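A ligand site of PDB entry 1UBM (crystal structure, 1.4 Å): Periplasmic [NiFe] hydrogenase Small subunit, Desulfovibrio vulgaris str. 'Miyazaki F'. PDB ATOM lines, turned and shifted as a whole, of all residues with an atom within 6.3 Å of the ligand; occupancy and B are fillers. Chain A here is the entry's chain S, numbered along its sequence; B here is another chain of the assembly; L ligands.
The side-chain sulfur of Cys 20 lies close to the backbone carbonyl oxygen of Tyr 111 (3.8 Å). The backbone NH (N) of Thr 113 lies within hydrogen-bond range of the backbone carbonyl oxygen (O) of Gly 149. The side-chain carboxylate (OE1) of Glu 75 sits close to the backbone NH (N) of Thr 18, at 3.4 Å. The side-chain sulfur (SG) of Cys 17 sits close to the backbone NH (N) of Gly 19, at 3.2 Å. The side-chain amide nitrogen (NE2) of Gln 121 sits close to the side-chain sulfur (SG) of Cys 114. The side-chain hydroxyl of Ser 21 is in hydrogen-bond range of the side-chain carboxylate of Glu 75 (2.6 Å). The backbone NH of Cys 20 sits at hydrogen-bond distance from the side-chain carboxylate of Glu 75 (3.1 Å). The backbone carbonyl oxygen (O) of Thr 113 sits at hydrogen-bond distance from the backbone NH (N) of Gly 119.
ND1 of His 217 of chain B lies close to S2 of the ligand (3.7 Å). The backbone NH (N) of Cys 17 sits close to a sulfur (S3) of the ligand, 3.5 Å away. A sulfur (S1) of the ligand sits close to the backbone NH (N) of Thr 113 (3.3 Å). S1 of the ligand lies close to N of Cys 114 (3.4 Å). The side-chain sulfur of Cys 150 is bound to an iron atom (FE3) of the ligand. An iron atom (FE2) of the ligand is bound by the side-chain sulfur of Cys 114, at 2.2 Å. The side-chain sulfur (SG) of Cys 17 binds an iron atom (FE1) of the ligand (2.3 Å). The side-chain sulfur (SG) of Cys 20 binds an iron atom (FE4) of the ligand (2.3 Å).
A sulfur (S1) of the ligand sits close to the backbone carbonyl oxygen (O) of Gly 149. The backbone nitrogen (N) of Pro 151 lies close to a sulfur (S2) of the ligand (3.7 Å). Merely in contact with the ligand: Arg 61 of chain B, Glu 16, Gly 112, Gly 19, Glu 75 and Val 120. Hydrophobic or aromatic side chains within 4 Å of the ligand: Val 120, Pro 151 and His 217 of chain B.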
ATOM      1  N   ALA A  15      21.695 -30.155  -2.284  1.00  0.00           N
ATOM      2  CA  ALA A  15      22.129 -29.381  -3.453  1.00  0.00           C
ATOM      3  C   ALA A  15      21.377 -28.050  -3.444  1.00  0.00           C
ATOM      4  O   ALA A  15      20.244 -27.966  -3.884  1.00  0.00           O
ATOM      5  CB  ALA A  15      21.975 -30.137  -4.756  1.00  0.00           C
ATOM      6  N   GLU A  16      22.012 -27.034  -2.915  1.00  0.00           N
ATOM      7  CA  GLU A  16      21.379 -25.771  -2.568  1.00  0.00           C
ATOM      8  C   GLU A  16      22.310 -24.572  -2.715  1.00  0.00           C
ATOM      9  O   GLU A  16      23.527 -24.780  -2.762  1.00  0.00           O
ATOM     10  CB  GLU A  16      20.853 -25.820  -1.117  1.00  0.00           C
ATOM     11  CG  GLU A  16      21.743 -26.438  -0.053  1.00  0.00           C
ATOM     12  CD  GLU A  16      22.743 -25.523   0.592  1.00  0.00           C
ATOM     13  OE1 GLU A  16      22.301 -24.366   0.797  1.00  0.00           O
ATOM     14  OE2 GLU A  16      23.909 -25.931   0.871  1.00  0.00           O
ATOM     15  N   CYS A  17      21.716 -23.383  -2.802  1.00  0.00           N
ATOM     16  CA  CYS A  17      22.499 -22.154  -2.907  1.00  0.00           C
ATOM     17  C   CYS A  17      22.546 -21.353  -1.585  1.00  0.00           C
ATOM     18  O   CYS A  17      23.207 -20.305  -1.520  1.00  0.00           O
ATOM     19  CB  CYS A  17      21.891 -21.245  -3.990  1.00  0.00           C
ATOM     20  SG  CYS A  17      20.402 -20.336  -3.457  1.00  0.00           S
ATOM     21  N   THR A  18      21.861 -21.836  -0.551  1.00  0.00           N
ATOM     22  CA  THR A  18      21.739 -21.290   0.799  1.00  0.00           C
ATOM     23  C   THR A  18      20.809 -20.071   0.836  1.00  0.00           C
ATOM     24  O   THR A  18      20.597 -19.461   1.898  1.00  0.00           O
ATOM     25  CB  THR A  18      23.149 -21.046   1.379  1.00  0.00           C
ATOM     26  OG1 THR A  18      23.908 -22.261   1.181  1.00  0.00           O
ATOM     27  CG2 THR A  18      23.167 -20.803   2.876  1.00  0.00           C
ATOM     28  N   GLY A  19      20.157 -19.746  -0.276  1.00  0.00           N
ATOM     29  CA  GLY A  19      19.120 -18.715  -0.346  1.00  0.00           C
ATOM     30  C   GLY A  19      17.942 -19.057   0.520  1.00  0.00           C
ATOM     31  O   GLY A  19      17.293 -18.189   1.111  1.00  0.00           O
ATOM     32  N   CYS A  20      17.625 -20.357   0.601  1.00  0.00           N
ATOM     33  CA  CYS A  20      16.526 -20.718   1.482  1.00  0.00           C
ATOM     34  C   CYS A  20      16.872 -20.502   2.946  1.00  0.00           C
ATOM     35  O   CYS A  20      16.090 -19.977   3.729  1.00  0.00           O
ATOM     36  CB  CYS A  20      16.103 -22.163   1.167  1.00  0.00           C
ATOM     37  SG  CYS A  20      15.149 -22.310  -0.335  1.00  0.00           S
ATOM     38  N   SER A  21      18.083 -20.886   3.363  1.00  0.00           N
ATOM     39  CA  SER A  21      18.501 -20.628   4.723  1.00  0.00           C
ATOM     40  C   SER A  21      18.477 -19.134   5.057  1.00  0.00           C
ATOM     41  O   SER A  21      18.062 -18.695   6.110  1.00  0.00           O
ATOM     42  CB  SER A  21      19.920 -21.136   4.970  1.00  0.00           C
ATOM     43  OG  SER A  21      19.950 -22.511   5.214  1.00  0.00           O
ATOM     44  N   GLU A  75      16.664 -28.333   2.831  1.00  0.00           N
ATOM     45  CA  GLU A  75      16.993 -27.378   1.767  1.00  0.00           C
ATOM     46  C   GLU A  75      17.838 -28.092   0.702  1.00  0.00           C
ATOM     47  O   GLU A  75      18.759 -28.835   1.017  1.00  0.00           O
ATOM     48  CB  GLU A  75      17.704 -26.152   2.317  1.00  0.00           C
ATOM     49  CG  GLU A  75      18.155 -25.046   1.357  1.00  0.00           C
ATOM     50  CD  GLU A  75      18.785 -23.862   2.077  1.00  0.00           C
ATOM     51  OE1 GLU A  75      19.230 -22.892   1.393  1.00  0.00           O
ATOM     52  OE2 GLU A  75      18.838 -23.907   3.338  1.00  0.00           O
ATOM     53  N   GLY A  76      17.481 -27.823  -0.545  1.00  0.00           N
ATOM     54  CA  GLY A  76      18.199 -28.343  -1.689  1.00  0.00           C
ATOM     55  C   GLY A  76      17.644 -29.630  -2.230  1.00  0.00           C
ATOM     56  O   GLY A  76      16.951 -30.422  -1.594  1.00  0.00           O
ATOM     57  N   GLY A  77      17.990 -29.877  -3.493  1.00  0.00           N
ATOM     58  CA  GLY A  77      17.657 -31.126  -4.134  1.00  0.00           C
ATOM     59  C   GLY A  77      18.695 -32.189  -3.805  1.00  0.00           C
ATOM     60  O   GLY A  77      19.794 -31.924  -3.313  1.00  0.00           O
ATOM     61  N   TYR A 111      11.836 -27.321   2.107  1.00  0.00           N
ATOM     62  CA  TYR A 111      11.785 -25.867   2.069  1.00  0.00           C
ATOM     63  C   TYR A 111      12.575 -25.416   0.859  1.00  0.00           C
ATOM     64  O   TYR A 111      13.769 -25.651   0.737  1.00  0.00           O
ATOM     65  CB  TYR A 111      12.336 -25.298   3.368  1.00  0.00           C
ATOM     66  CG  TYR A 111      12.199 -23.790   3.461  1.00  0.00           C
ATOM     67  CD1 TYR A 111      10.918 -23.220   3.440  1.00  0.00           C
ATOM     68  CD2 TYR A 111      13.307 -22.946   3.536  1.00  0.00           C
ATOM     69  CE1 TYR A 111      10.730 -21.860   3.513  1.00  0.00           C
ATOM     70  CE2 TYR A 111      13.119 -21.579   3.601  1.00  0.00           C
ATOM     71  CZ  TYR A 111      11.856 -21.037   3.596  1.00  0.00           C
ATOM     72  OH  TYR A 111      11.699 -19.673   3.661  1.00  0.00           O
ATOM     73  N   GLY A 112      11.858 -24.783  -0.068  1.00  0.00           N
ATOM     74  CA  GLY A 112      12.334 -24.239  -1.294  1.00  0.00           C
ATOM     75  C   GLY A 112      12.079 -25.162  -2.480  1.00  0.00           C
ATOM     76  O   GLY A 112      12.009 -26.389  -2.340  1.00  0.00           O
ATOM     77  N   THR A 113      11.958 -24.562  -3.664  1.00  0.00           N
ATOM     78  CA  THR A 113      11.683 -25.337  -4.885  1.00  0.00           C
ATOM     79  C   THR A 113      12.713 -26.408  -5.159  1.00  0.00           C
ATOM     80  O   THR A 113      12.385 -27.465  -5.734  1.00  0.00           O
ATOM     81  CB  THR A 113      11.563 -24.334  -6.023  1.00  0.00           C
ATOM     82  OG1 THR A 113      10.382 -23.561  -5.703  1.00  0.00           O
ATOM     83  CG2 THR A 113      11.365 -25.006  -7.376  1.00  0.00           C
ATOM     84  N   CYS A 114      13.964 -26.237  -4.789  1.00  0.00           N
ATOM     85  CA  CYS A 114      14.962 -27.339  -4.959  1.00  0.00           C
ATOM     86  C   CYS A 114      14.541 -28.545  -4.132  1.00  0.00           C
ATOM     87  O   CYS A 114      14.502 -29.640  -4.660  1.00  0.00           O
ATOM     88  CB  CYS A 114      16.381 -26.937  -4.586  1.00  0.00           C
ATOM     89  SG  CYS A 114      17.063 -25.560  -5.584  1.00  0.00           S
ATOM     90  N   ALA A 115      14.252 -28.349  -2.845  1.00  0.00           N
ATOM     91  CA  ALA A 115      13.904 -29.514  -2.045  1.00  0.00           C
ATOM     92  C   ALA A 115      12.517 -30.036  -2.386  1.00  0.00           C
ATOM     93  O   ALA A 115      12.267 -31.242  -2.302  1.00  0.00           O
ATOM     94  CB  ALA A 115      13.968 -29.189  -0.557  1.00  0.00           C
ATOM     95  N   GLY A 119      14.458 -28.230  -8.438  1.00  0.00           N
ATOM     96  CA  GLY A 119      14.997 -26.906  -8.632  1.00  0.00           C
ATOM     97  C   GLY A 119      16.058 -26.752  -9.684  1.00  0.00           C
ATOM     98  O   GLY A 119      16.122 -27.458 -10.677  1.00  0.00           O
ATOM     99  N   VAL A 120      16.908 -25.756  -9.420  1.00  0.00           N
ATOM    100  CA  VAL A 120      17.746 -25.224 -10.496  1.00  0.00           C
ATOM    101  C   VAL A 120      18.683 -26.283 -11.011  1.00  0.00           C
ATOM    102  O   VAL A 120      18.871 -26.379 -12.221  1.00  0.00           O
ATOM    103  CB  VAL A 120      18.480 -23.944 -10.029  1.00  0.00           C
ATOM    104  CG1 VAL A 120      19.518 -24.208  -8.952  1.00  0.00           C
ATOM    105  CG2 VAL A 120      19.090 -23.222 -11.233  1.00  0.00           C
ATOM    106  N   GLN A 121      19.255 -27.096 -10.135  1.00  0.00           N
ATOM    107  CA  GLN A 121      20.185 -28.117 -10.632  1.00  0.00           C
ATOM    108  C   GLN A 121      19.438 -29.262 -11.325  1.00  0.00           C
ATOM    109  O   GLN A 121      20.060 -30.067 -12.035  1.00  0.00           O
ATOM    110  CB  GLN A 121      21.061 -28.663  -9.496  1.00  0.00           C
ATOM    111  CG  GLN A 121      20.291 -29.239  -8.310  1.00  0.00           C
ATOM    112  CD  GLN A 121      19.935 -28.142  -7.335  1.00  0.00           C
ATOM    113  OE1 GLN A 121      20.795 -27.285  -7.093  1.00  0.00           O
ATOM    114  NE2 GLN A 121      18.732 -28.100  -6.789  1.00  0.00           N
ATOM    115  N   GLY A 149       9.064 -22.110  -3.641  1.00  0.00           N
ATOM    116  CA  GLY A 149       9.579 -20.808  -3.932  1.00  0.00           C
ATOM    117  C   GLY A 149      11.111 -20.838  -3.960  1.00  0.00           C
ATOM    118  O   GLY A 149      11.732 -21.743  -3.417  1.00  0.00           O
ATOM    119  N   CYS A 150      11.664 -19.778  -4.577  1.00  0.00           N
ATOM    120  CA  CYS A 150      13.094 -19.781  -4.847  1.00  0.00           C
ATOM    121  C   CYS A 150      13.731 -18.440  -4.490  1.00  0.00           C
ATOM    122  O   CYS A 150      14.179 -17.666  -5.348  1.00  0.00           O
ATOM    123  CB  CYS A 150      13.357 -20.163  -6.301  1.00  0.00           C
ATOM    124  SG  CYS A 150      15.035 -20.587  -6.685  1.00  0.00           S
ATOM    125  N   PRO A 151      13.799 -18.156  -3.190  1.00  0.00           N
ATOM    126  CA  PRO A 151      13.331 -18.975  -2.073  1.00  0.00           C
ATOM    127  C   PRO A 151      11.890 -18.604  -1.695  1.00  0.00           C
ATOM    128  O   PRO A 151      11.295 -17.629  -2.167  1.00  0.00           O
ATOM    129  CB  PRO A 151      14.249 -18.562  -0.937  1.00  0.00           C
ATOM    130  CG  PRO A 151      14.456 -17.100  -1.201  1.00  0.00           C
ATOM    131  CD  PRO A 151      14.468 -16.946  -2.694  1.00  0.00           C
ATOM    132  N   PRO A 152      11.324 -19.464  -0.863  1.00  0.00           N
ATOM    133  CA  PRO A 152       9.956 -19.206  -0.419  1.00  0.00           C
ATOM    134  C   PRO A 152       9.908 -17.994   0.510  1.00  0.00           C
ATOM    135  O   PRO A 152      10.924 -17.516   1.006  1.00  0.00           O
ATOM    136  CB  PRO A 152       9.581 -20.461   0.383  1.00  0.00           C
ATOM    137  CG  PRO A 152      10.611 -21.505   0.028  1.00  0.00           C
ATOM    138  CD  PRO A 152      11.841 -20.700  -0.286  1.00  0.00           C
ATOM    139  N   TRP A 258      12.116 -23.843 -14.130  1.00  0.00           N
ATOM    140  CA  TRP A 258      13.277 -23.472 -14.935  1.00  0.00           C
ATOM    141  C   TRP A 258      13.100 -23.837 -16.410  1.00  0.00           C
ATOM    142  O   TRP A 258      13.609 -23.172 -17.315  1.00  0.00           O
ATOM    143  CB  TRP A 258      14.536 -24.153 -14.384  1.00  0.00           C
ATOM    144  CG  TRP A 258      14.789 -23.707 -12.968  1.00  0.00           C
ATOM    145  CD1 TRP A 258      14.594 -24.370 -11.800  1.00  0.00           C
ATOM    146  CD2 TRP A 258      15.312 -22.409 -12.627  1.00  0.00           C
ATOM    147  NE1 TRP A 258      14.959 -23.562 -10.755  1.00  0.00           N
ATOM    148  CE2 TRP A 258      15.404 -22.364 -11.212  1.00  0.00           C
ATOM    149  CE3 TRP A 258      15.707 -21.291 -13.360  1.00  0.00           C
ATOM    150  CZ2 TRP A 258      15.869 -21.237 -10.547  1.00  0.00           C
ATOM    151  CZ3 TRP A 258      16.172 -20.170 -12.687  1.00  0.00           C
ATOM    152  CH2 TRP A 258      16.252 -20.141 -11.299  1.00  0.00           C
ATOM    153  N   ARG B  41      26.777 -28.759  -8.999  1.00  0.00           N
ATOM    154  CA  ARG B  41      25.437 -28.608  -9.562  1.00  0.00           C
ATOM    155  C   ARG B  41      25.464 -28.516 -11.091  1.00  0.00           C
ATOM    156  O   ARG B  41      24.561 -29.074 -11.737  1.00  0.00           O
ATOM    157  CB  ARG B  41      24.682 -27.418  -8.957  1.00  0.00           C
ATOM    158  CG  ARG B  41      24.314 -27.628  -7.515  1.00  0.00           C
ATOM    159  CD  ARG B  41      23.774 -26.400  -6.790  1.00  0.00           C
ATOM    160  NE  ARG B  41      24.786 -25.352  -6.747  1.00  0.00           N
ATOM    161  CZ  ARG B  41      24.555 -24.037  -6.662  1.00  0.00           C
ATOM    162  NH1 ARG B  41      23.297 -23.574  -6.588  1.00  0.00           N
ATOM    163  NH2 ARG B  41      25.600 -23.209  -6.656  1.00  0.00           N
ATOM    164  N   ARG B  61      21.025 -18.054  -8.767  1.00  0.00           N
ATOM    165  CA  ARG B  61      20.860 -19.203  -7.880  1.00  0.00           C
ATOM    166  C   ARG B  61      22.200 -19.959  -7.686  1.00  0.00           C
ATOM    167  O   ARG B  61      22.218 -21.033  -7.065  1.00  0.00           O
ATOM    168  CB  ARG B  61      19.750 -20.152  -8.300  1.00  0.00           C
ATOM    169  CG  ARG B  61      18.364 -19.720  -7.922  1.00  0.00           C
ATOM    170  CD  ARG B  61      17.930 -18.433  -8.569  1.00  0.00           C
ATOM    171  NE  ARG B  61      16.589 -18.076  -8.107  1.00  0.00           N
ATOM    172  CZ  ARG B  61      15.892 -17.019  -8.464  1.00  0.00           C
ATOM    173  NH1 ARG B  61      16.404 -16.183  -9.371  1.00  0.00           N
ATOM    174  NH2 ARG B  61      14.692 -16.789  -7.957  1.00  0.00           N
ATOM    175  N   GLY B  64      22.835 -17.857  -2.634  1.00  0.00           N
ATOM    176  CA  GLY B  64      21.855 -17.007  -1.957  1.00  0.00           C
ATOM    177  C   GLY B  64      22.381 -16.213  -0.786  1.00  0.00           C
ATOM    178  O   GLY B  64      21.626 -15.422  -0.185  1.00  0.00           O
ATOM    179  N   PRO B 216      16.098 -12.923  -0.070  1.00  0.00           N
ATOM    180  CA  PRO B 216      17.036 -13.203  -1.149  1.00  0.00           C
ATOM    181  C   PRO B 216      16.421 -13.272  -2.544  1.00  0.00           C
ATOM    182  O   PRO B 216      15.237 -13.499  -2.776  1.00  0.00           O
ATOM    183  CB  PRO B 216      17.597 -14.603  -0.835  1.00  0.00           C
ATOM    184  CG  PRO B 216      17.269 -14.817   0.606  1.00  0.00           C
ATOM    185  CD  PRO B 216      15.918 -14.131   0.780  1.00  0.00           C
ATOM    186  N   HIS B 217      17.323 -13.116  -3.487  1.00  0.00           N
ATOM    187  CA  HIS B 217      17.214 -13.247  -4.921  1.00  0.00           C
ATOM    188  C   HIS B 217      16.327 -12.139  -5.478  1.00  0.00           C
ATOM    189  O   HIS B 217      15.134 -12.224  -5.723  1.00  0.00           O
ATOM    190  CB  HIS B 217      16.712 -14.659  -5.316  1.00  0.00           C
ATOM    191  CG  HIS B 217      17.717 -15.738  -5.106  1.00  0.00           C
ATOM    192  ND1 HIS B 217      17.668 -17.078  -4.927  1.00  0.00           N
ATOM    193  CD2 HIS B 217      19.040 -15.604  -5.138  1.00  0.00           C
ATOM    194  CE1 HIS B 217      18.882 -17.640  -4.799  1.00  0.00           C
ATOM    195  NE2 HIS B 217      19.804 -16.693  -4.908  1.00  0.00           N
HETATM  196 FE1  LIG L   1      18.547 -21.625  -3.687  1.00  0.00          FE
HETATM  197 FE2  LIG L   1      17.124 -23.773  -4.306  1.00  0.00          FE
HETATM  198 FE3  LIG L   1      16.151 -21.399  -4.875  1.00  0.00          FE
HETATM  199 FE4  LIG L   1      16.327 -22.184  -2.260  1.00  0.00          FE
HETATM  200  S1  LIG L   1      14.943 -23.113  -3.856  1.00  0.00           S
HETATM  201  S2  LIG L   1      16.846 -20.188  -3.172  1.00  0.00           S
HETATM  202  S3  LIG L   1      18.253 -23.496  -2.352  1.00  0.00           S
HETATM  203  S4  LIG L   1      18.106 -22.324  -5.800  1.00  0.00           S
